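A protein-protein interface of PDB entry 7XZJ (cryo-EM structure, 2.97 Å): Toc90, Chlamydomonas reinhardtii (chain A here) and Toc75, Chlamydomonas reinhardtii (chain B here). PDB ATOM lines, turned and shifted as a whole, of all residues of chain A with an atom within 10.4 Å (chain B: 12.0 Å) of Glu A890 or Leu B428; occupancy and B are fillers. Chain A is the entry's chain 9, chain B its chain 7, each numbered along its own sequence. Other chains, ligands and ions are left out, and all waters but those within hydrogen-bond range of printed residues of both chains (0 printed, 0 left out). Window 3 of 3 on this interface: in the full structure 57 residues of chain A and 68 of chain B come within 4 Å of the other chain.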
ATOM      1  N   GLY A 863     -14.223   3.368  -5.066  1.00  0.00           N
ATOM      2  CA  GLY A 863     -13.851   2.134  -4.348  1.00  0.00           C
ATOM      3  C   GLY A 863     -13.606   0.985  -5.307  1.00  0.00           C
ATOM      4  O   GLY A 863     -14.353   0.880  -6.292  1.00  0.00           O
ATOM      5  N   TYR A 864     -12.601   0.152  -5.029  1.00  0.00           N
ATOM      6  CA  TYR A 864     -12.271  -0.968  -5.893  1.00  0.00           C
ATOM      7  C   TYR A 864     -11.908  -2.183  -5.051  1.00  0.00           C
ATOM      8  O   TYR A 864     -11.532  -2.070  -3.882  1.00  0.00           O
ATOM      9  CB  TYR A 864     -11.121  -0.620  -6.848  1.00  0.00           C
ATOM     10  CG  TYR A 864      -9.797  -0.360  -6.167  1.00  0.00           C
ATOM     11  CD1 TYR A 864      -9.489   0.893  -5.659  1.00  0.00           C
ATOM     12  CD2 TYR A 864      -8.848  -1.367  -6.049  1.00  0.00           C
ATOM     13  CE1 TYR A 864      -8.276   1.133  -5.044  1.00  0.00           C
ATOM     14  CE2 TYR A 864      -7.635  -1.136  -5.438  1.00  0.00           C
ATOM     15  CZ  TYR A 864      -7.353   0.115  -4.937  1.00  0.00           C
ATOM     16  OH  TYR A 864      -6.143   0.346  -4.326  1.00  0.00           O
ATOM     17  N   GLY A 865     -12.031  -3.349  -5.666  1.00  0.00           N
ATOM     18  CA  GLY A 865     -11.727  -4.599  -4.995  1.00  0.00           C
ATOM     19  C   GLY A 865     -11.038  -5.567  -5.932  1.00  0.00           C
ATOM     20  O   GLY A 865     -11.231  -5.535  -7.154  1.00  0.00           O
ATOM     21  N   ASP A 884      -9.618 -12.201  -1.107  1.00  0.00           N
ATOM     22  CA  ASP A 884     -10.290 -10.981  -1.526  1.00  0.00           C
ATOM     23  C   ASP A 884      -9.717  -9.805  -0.753  1.00  0.00           C
ATOM     24  O   ASP A 884      -9.558  -9.879   0.470  1.00  0.00           O
ATOM     25  CB  ASP A 884     -11.802 -11.082  -1.312  1.00  0.00           C
ATOM     26  CG  ASP A 884     -12.529  -9.814  -1.706  1.00  0.00           C
ATOM     27  OD1 ASP A 884     -12.331  -9.347  -2.849  1.00  0.00           O
ATOM     28  OD2 ASP A 884     -13.302  -9.287  -0.880  1.00  0.00           O
ATOM     29  N   TYR A 885      -9.400  -8.726  -1.463  1.00  0.00           N
ATOM     30  CA  TYR A 885      -8.877  -7.511  -0.853  1.00  0.00           C
ATOM     31  C   TYR A 885      -9.790  -6.346  -1.196  1.00  0.00           C
ATOM     32  O   TYR A 885     -10.083  -6.106  -2.376  1.00  0.00           O
ATOM     33  CB  TYR A 885      -7.448  -7.224  -1.315  1.00  0.00           C
ATOM     34  CG  TYR A 885      -6.961  -5.856  -0.896  1.00  0.00           C
ATOM     35  CD1 TYR A 885      -6.773  -5.547   0.444  1.00  0.00           C
ATOM     36  CD2 TYR A 885      -6.695  -4.873  -1.837  1.00  0.00           C
ATOM     37  CE1 TYR A 885      -6.334  -4.299   0.835  1.00  0.00           C
ATOM     38  CE2 TYR A 885      -6.253  -3.620  -1.456  1.00  0.00           C
ATOM     39  CZ  TYR A 885      -6.074  -3.339  -0.118  1.00  0.00           C
ATOM     40  OH  TYR A 885      -5.635  -2.096   0.274  1.00  0.00           O
ATOM     41  N   VAL A 886     -10.232  -5.630  -0.166  1.00  0.00           N
ATOM     42  CA  VAL A 886     -10.999  -4.400  -0.319  1.00  0.00           C
ATOM     43  C   VAL A 886     -10.149  -3.255   0.216  1.00  0.00           C
ATOM     44  O   VAL A 886      -9.829  -3.210   1.412  1.00  0.00           O
ATOM     45  CB  VAL A 886     -12.350  -4.475   0.407  1.00  0.00           C
ATOM     46  CG1 VAL A 886     -13.141  -3.197   0.189  1.00  0.00           C
ATOM     47  CG2 VAL A 886     -13.139  -5.680  -0.075  1.00  0.00           C
ATOM     48  N   ALA A 887      -9.779  -2.334  -0.677  1.00  0.00           N
ATOM     49  CA  ALA A 887      -8.935  -1.210  -0.290  1.00  0.00           C
ATOM     50  C   ALA A 887      -9.698  -0.178   0.528  1.00  0.00           C
ATOM     51  O   ALA A 887      -9.117   0.461   1.415  1.00  0.00           O
ATOM     52  CB  ALA A 887      -8.330  -0.558  -1.533  1.00  0.00           C
ATOM     53  N   ALA A 888     -10.991   0.005   0.245  1.00  0.00           N
ATOM     54  CA  ALA A 888     -11.768   1.034   0.931  1.00  0.00           C
ATOM     55  C   ALA A 888     -11.833   0.790   2.431  1.00  0.00           C
ATOM     56  O   ALA A 888     -11.892   1.746   3.212  1.00  0.00           O
ATOM     57  CB  ALA A 888     -13.176   1.108   0.340  1.00  0.00           C
ATOM     58  N   SER A 889     -11.753  -0.484   2.834  1.00  0.00           N
ATOM     59  CA  SER A 889     -11.851  -0.838   4.275  1.00  0.00           C
ATOM     60  C   SER A 889     -10.528  -1.425   4.776  1.00  0.00           C
ATOM     61  O   SER A 889     -10.447  -1.725   5.983  1.00  0.00           O
ATOM     62  CB  SER A 889     -12.983  -1.801   4.505  1.00  0.00           C
ATOM     63  OG  SER A 889     -12.728  -3.035   3.851  1.00  0.00           O
ATOM     64  N   GLU A 890      -9.552  -1.606   3.882  1.00  0.00           N
ATOM     65  CA  GLU A 890      -8.235  -2.185   4.266  1.00  0.00           C
ATOM     66  C   GLU A 890      -8.461  -3.531   4.970  1.00  0.00           C
ATOM     67  O   GLU A 890      -7.845  -3.761   6.027  1.00  0.00           O
ATOM     68  CB  GLU A 890      -7.420  -1.192   5.100  1.00  0.00           C
ATOM     69  CG  GLU A 890      -5.928  -1.247   4.822  1.00  0.00           C
ATOM     70  CD  GLU A 890      -5.158  -2.276   5.633  1.00  0.00           C
ATOM     71  OE1 GLU A 890      -5.412  -2.376   6.849  1.00  0.00           O
ATOM     72  OE2 GLU A 890      -4.316  -2.982   5.044  1.00  0.00           O
ATOM     73  N   SER A 891      -9.341  -4.370   4.418  1.00  0.00           N
ATOM     74  CA  SER A 891      -9.623  -5.698   5.022  1.00  0.00           C
ATOM     75  C   SER A 891      -9.228  -6.805   4.041  1.00  0.00           C
ATOM     76  O   SER A 891      -9.553  -6.667   2.845  1.00  0.00           O
ATOM     77  CB  SER A 891     -11.073  -5.805   5.396  1.00  0.00           C
ATOM     78  OG  SER A 891     -11.459  -4.719   6.226  1.00  0.00           O
ATOM     79  N   VAL A 892      -8.561  -7.858   4.524  1.00  0.00           N
ATOM     80  CA  VAL A 892      -8.233  -9.005   3.628  1.00  0.00           C
ATOM     81  C   VAL A 892      -9.015 -10.235   4.085  1.00  0.00           C
ATOM     82  O   VAL A 892      -8.950 -10.557   5.283  1.00  0.00           O
ATOM     83  CB  VAL A 892      -6.724  -9.298   3.627  1.00  0.00           C
ATOM     84  CG1 VAL A 892      -6.413 -10.648   3.001  1.00  0.00           C
ATOM     85  CG2 VAL A 892      -5.936  -8.191   2.946  1.00  0.00           C
ATOM     86  N   PHE A 893      -9.716 -10.895   3.164  1.00  0.00           N
ATOM     87  CA  PHE A 893     -10.425 -12.117   3.512  1.00  0.00           C
ATOM     88  C   PHE A 893      -9.769 -13.294   2.806  1.00  0.00           C
ATOM     89  O   PHE A 893      -9.431 -13.207   1.621  1.00  0.00           O
ATOM     90  CB  PHE A 893     -11.902 -12.039   3.115  1.00  0.00           C
ATOM     91  CG  PHE A 893     -12.647 -10.907   3.759  1.00  0.00           C
ATOM     92  CD1 PHE A 893     -12.637  -9.646   3.193  1.00  0.00           C
ATOM     93  CD2 PHE A 893     -13.370 -11.109   4.922  1.00  0.00           C
ATOM     94  CE1 PHE A 893     -13.326  -8.603   3.779  1.00  0.00           C
ATOM     95  CE2 PHE A 893     -14.062 -10.070   5.512  1.00  0.00           C
ATOM     96  CZ  PHE A 893     -14.039  -8.815   4.940  1.00  0.00           C
ATOM     97  N   TRP B 424     -11.143 -16.495   7.029  1.00  0.00           N
ATOM     98  CA  TRP B 424     -10.197 -15.614   7.766  1.00  0.00           C
ATOM     99  C   TRP B 424     -10.490 -14.145   7.448  1.00  0.00           C
ATOM    100  O   TRP B 424     -11.047 -13.880   6.367  1.00  0.00           O
ATOM    101  CB  TRP B 424      -8.740 -15.973   7.450  1.00  0.00           C
ATOM    102  CG  TRP B 424      -8.258 -17.213   8.136  1.00  0.00           C
ATOM    103  CD1 TRP B 424      -7.882 -17.337   9.443  1.00  0.00           C
ATOM    104  CD2 TRP B 424      -8.101 -18.516   7.548  1.00  0.00           C
ATOM    105  NE1 TRP B 424      -7.503 -18.625   9.707  1.00  0.00           N
ATOM    106  CE2 TRP B 424      -7.627 -19.372   8.565  1.00  0.00           C
ATOM    107  CE3 TRP B 424      -8.316 -19.040   6.269  1.00  0.00           C
ATOM    108  CZ2 TRP B 424      -7.362 -20.720   8.335  1.00  0.00           C
ATOM    109  CZ3 TRP B 424      -8.054 -20.372   6.045  1.00  0.00           C
ATOM    110  CH2 TRP B 424      -7.583 -21.198   7.065  1.00  0.00           C
ATOM    111  N   SER B 425     -10.131 -13.237   8.359  1.00  0.00           N
ATOM    112  CA  SER B 425     -10.308 -11.780   8.116  1.00  0.00           C
ATOM    113  C   SER B 425      -9.095 -11.050   8.696  1.00  0.00           C
ATOM    114  O   SER B 425      -9.174 -10.623   9.864  1.00  0.00           O
ATOM    115  CB  SER B 425     -11.594 -11.278   8.717  1.00  0.00           C
ATOM    116  OG  SER B 425     -11.780  -9.901   8.424  1.00  0.00           O
ATOM    117  N   PHE B 426      -8.021 -10.915   7.915  1.00  0.00           N
ATOM    118  CA  PHE B 426      -6.772 -10.319   8.453  1.00  0.00           C
ATOM    119  C   PHE B 426      -6.740  -8.815   8.184  1.00  0.00           C
ATOM    120  O   PHE B 426      -6.990  -8.407   7.036  1.00  0.00           O
ATOM    121  CB  PHE B 426      -5.551 -10.976   7.808  1.00  0.00           C
ATOM    122  CG  PHE B 426      -5.340 -12.425   8.161  1.00  0.00           C
ATOM    123  CD1 PHE B 426      -4.970 -12.795   9.443  1.00  0.00           C
ATOM    124  CD2 PHE B 426      -5.494 -13.417   7.206  1.00  0.00           C
ATOM    125  CE1 PHE B 426      -4.768 -14.128   9.766  1.00  0.00           C
ATOM    126  CE2 PHE B 426      -5.288 -14.748   7.529  1.00  0.00           C
ATOM    127  CZ  PHE B 426      -4.927 -15.102   8.808  1.00  0.00           C
ATOM    128  N   GLN B 427      -6.418  -8.023   9.214  1.00  0.00           N
ATOM    129  CA  GLN B 427      -6.319  -6.544   9.068  1.00  0.00           C
ATOM    130  C   GLN B 427      -4.908  -6.116   9.480  1.00  0.00           C
ATOM    131  O   GLN B 427      -4.546  -6.350  10.649  1.00  0.00           O
ATOM    132  CB  GLN B 427      -7.324  -5.860   9.995  1.00  0.00           C
ATOM    133  CG  GLN B 427      -8.656  -6.587  10.103  1.00  0.00           C
ATOM    134  CD  GLN B 427      -9.524  -6.352   8.892  1.00  0.00           C
ATOM    135  OE1 GLN B 427     -10.139  -7.273   8.359  1.00  0.00           O
ATOM    136  NE2 GLN B 427      -9.568  -5.109   8.445  1.00  0.00           N
ATOM    137  N   LEU B 428      -4.141  -5.522   8.561  1.00  0.00           N
ATOM    138  CA  LEU B 428      -2.737  -5.143   8.874  1.00  0.00           C
ATOM    139  C   LEU B 428      -2.563  -3.629   8.750  1.00  0.00           C
ATOM    140  O   LEU B 428      -2.820  -3.102   7.656  1.00  0.00           O
ATOM    141  CB  LEU B 428      -1.816  -5.851   7.877  1.00  0.00           C
ATOM    142  N   LYS B 429      -2.078  -2.965   9.804  1.00  0.00           N
ATOM    143  CA  LYS B 429      -1.796  -1.509   9.696  1.00  0.00           C
ATOM    144  C   LYS B 429      -0.707  -1.321   8.638  1.00  0.00           C
ATOM    145  O   LYS B 429      -0.839  -0.393   7.816  1.00  0.00           O
ATOM    146  CB  LYS B 429      -1.350  -0.951  11.051  1.00  0.00           C
ATOM    147  N   ASN B 430       0.319  -2.177   8.656  1.00  0.00           N
ATOM    148  CA  ASN B 430       1.382  -2.129   7.618  1.00  0.00           C
ATOM    149  C   ASN B 430       1.766  -3.571   7.274  1.00  0.00           C
ATOM    150  O   ASN B 430       1.731  -4.415   8.190  1.00  0.00           O
ATOM    151  CB  ASN B 430       2.596  -1.328   8.097  1.00  0.00           C
ATOM    152  CG  ASN B 430       3.512  -0.899   6.970  1.00  0.00           C
ATOM    153  OD1 ASN B 430       4.711  -0.723   7.171  1.00  0.00           O
ATOM    154  ND2 ASN B 430       2.958  -0.731   5.780  1.00  0.00           N
ATOM    155  N   GLY B 431       2.115  -3.845   6.012  1.00  0.00           N
ATOM    156  CA  GLY B 431       2.579  -5.196   5.646  1.00  0.00           C
ATOM    157  C   GLY B 431       1.538  -6.254   5.967  1.00  0.00           C
ATOM    158  O   GLY B 431       0.397  -6.122   5.485  1.00  0.00           O
ATOM    159  N   ILE B 432       1.920  -7.269   6.747  1.00  0.00           N
ATOM    160  CA  ILE B 432       0.974  -8.351   7.152  1.00  0.00           C
ATOM    161  C   ILE B 432       0.748  -8.231   8.663  1.00  0.00           C
ATOM    162  O   ILE B 432       1.634  -7.673   9.341  1.00  0.00           O
ATOM    163  CB  ILE B 432       1.540  -9.731   6.761  1.00  0.00           C
ATOM    164  N   PRO B 433      -0.380  -8.717   9.228  1.00  0.00           N
ATOM    165  CA  PRO B 433      -0.582  -8.685  10.678  1.00  0.00           C
ATOM    166  C   PRO B 433       0.417  -9.626  11.370  1.00  0.00           C
ATOM    167  O   PRO B 433       0.760 -10.644  10.792  1.00  0.00           O
ATOM    168  CB  PRO B 433      -2.023  -9.178  10.869  1.00  0.00           C
ATOM    169  CG  PRO B 433      -2.313  -9.988   9.625  1.00  0.00           C
ATOM    170  CD  PRO B 433      -1.513  -9.324   8.522  1.00  0.00           C
ATOM    171  N   SER B 434       0.856  -9.265  12.579  1.00  0.00           N
ATOM    172  CA  SER B 434       1.843 -10.104  13.307  1.00  0.00           C
ATOM    173  C   SER B 434       1.224 -11.482  13.547  1.00  0.00           C
ATOM    174  O   SER B 434       0.028 -11.536  13.896  1.00  0.00           O
ATOM    175  CB  SER B 434       2.252  -9.456  14.602  1.00  0.00           C
ATOM    176  OG  SER B 434       3.105 -10.313  15.346  1.00  0.00           O
ATOM    177  N   ILE B 435       2.008 -12.551  13.374  1.00  0.00           N
ATOM    178  CA  ILE B 435       1.417 -13.917  13.492  1.00  0.00           C
ATOM    179  C   ILE B 435       0.897 -14.087  14.921  1.00  0.00           C
ATOM    180  O   ILE B 435       1.674 -13.840  15.864  1.00  0.00           O
ATOM    181  CB  ILE B 435       2.460 -14.995  13.134  1.00  0.00           C
ATOM    182  N   ASN B 436      -0.360 -14.517  15.062  1.00  0.00           N
ATOM    183  CA  ASN B 436      -0.969 -14.716  16.403  1.00  0.00           C
ATOM    184  C   ASN B 436      -1.899 -15.928  16.338  1.00  0.00           C
ATOM    185  O   ASN B 436      -2.473 -16.165  15.258  1.00  0.00           O
ATOM    186  CB  ASN B 436      -1.757 -13.483  16.854  1.00  0.00           C
ATOM    187  CG  ASN B 436      -0.879 -12.312  17.241  1.00  0.00           C
ATOM    188  OD1 ASN B 436       0.058 -12.463  18.022  1.00  0.00           O
ATOM    189  ND2 ASN B 436      -1.181 -11.139  16.708  1.00  0.00           N
ATOM    190  N   GLN B 438      -4.712 -16.073  17.890  1.00  0.00           N
ATOM    191  CA  GLN B 438      -6.057 -15.451  17.767  1.00  0.00           C
ATOM    192  C   GLN B 438      -6.329 -15.095  16.299  1.00  0.00           C
ATOM    193  O   GLN B 438      -7.475 -15.294  15.854  1.00  0.00           O
ATOM    194  CB  GLN B 438      -6.194 -14.254  18.715  1.00  0.00           C
ATOM    195  CG  GLN B 438      -5.070 -13.234  18.607  1.00  0.00           C
ATOM    196  CD  GLN B 438      -5.438 -12.055  17.740  1.00  0.00           C
ATOM    197  OE1 GLN B 438      -6.578 -11.913  17.302  1.00  0.00           O
ATOM    198  NE2 GLN B 438      -4.468 -11.193  17.484  1.00  0.00           N
ATOM    199  N   SER B 439      -5.319 -14.592  15.578  1.00  0.00           N
ATOM    200  CA  SER B 439      -5.548 -14.165  14.173  1.00  0.00           C
ATOM    201  C   SER B 439      -5.663 -15.400  13.275  1.00  0.00           C
ATOM    202  O   SER B 439      -6.217 -15.269  12.171  1.00  0.00           O
ATOM    203  CB  SER B 439      -4.451 -13.246  13.704  1.00  0.00           C
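N of Phe B426 lies within hydrogen-bond range of O of Val A892.
NE2 of Gln B427 lies within hydrogen-bond range of O of Glu A890, at 3.3 Å.
NE2 of Gln B427 sits at hydrogen-bond distance from OG of Ser A891 (2.9 Å).
The backbone carbonyl oxygen (O) of Leu B428 lies close to the side-chain carboxylate (OE1) of Glu A890, 2.8 Å away.
The side-chain hydroxyl (OG) of Ser B425 is in hydrogen-bond range of the side-chain amide oxygen (OE1) of Gln B427, at 3.1 Å.
The backbone carbonyl oxygen (O) of Asp A884 sits at hydrogen-bond distance from the backbone NH (N) of Phe A893 (2.9 Å).
The backbone NH (N) of Val A886 is in hydrogen-bond range of the backbone carbonyl oxygen (O) of Ser A891 (3.3 Å).
The side-chain hydroxyl of Ser A891 sits at hydrogen-bond distance from the backbone carbonyl oxygen of Ser A889, 3.2 Å away.
Among the printed residues, merely in contact across the chains: Val A892 with Ser B425 (3.4 Å), Phe A893 with Trp B424 (3.4 Å) and Phe A893 with Ser B425 (3.7 Å).
Of chain B, only Gln B427 (3.3 Å) and Leu B428 (2.8 Å) come within 4 Å of Glu A890.
Leu B428 touches just one residue of chain A: Glu A890 (2.8 Å).
No residue of chain B comes within 4 Å of Ala A887.
No residue of chain B comes within 4 Å of Ser A889.
Of the printed residues of chain B, Ser A891 touches Gln B427.
Val A892 touches just these residues of chain B: Ser B425 and Phe B426.
No residue of chain A comes within 4 Å of Lys B429.
No residue of chain A comes within 4 Å of Gly B431.
No residue of chain A comes within 4 Å of Ile B432.
Pro B433 touches none of the printed residues of chain A.
Of the printed residues of chain A, Ser B425 touches Val A892 and Phe A893.
Of the printed residues of chain A, Trp B424 touches Phe A893.
Of the printed residues of chain A, Phe B426 touches Val A892 (2.8 Å).
Of the printed residues of chain B, Phe A893 touches Trp B424 and Ser B425.
Asn B436 touches none of the printed residues of chain A.
The nearest residue of chain B that does not touch Glu A890 is Lys B429 (4.5 Å).
Hydrophobic or aromatic side chains of chain A that line the printed part of chain B: Val A892 and Phe A893.
Of the 15 printed residues of chain B, 5 touch a printed residue of chain A.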
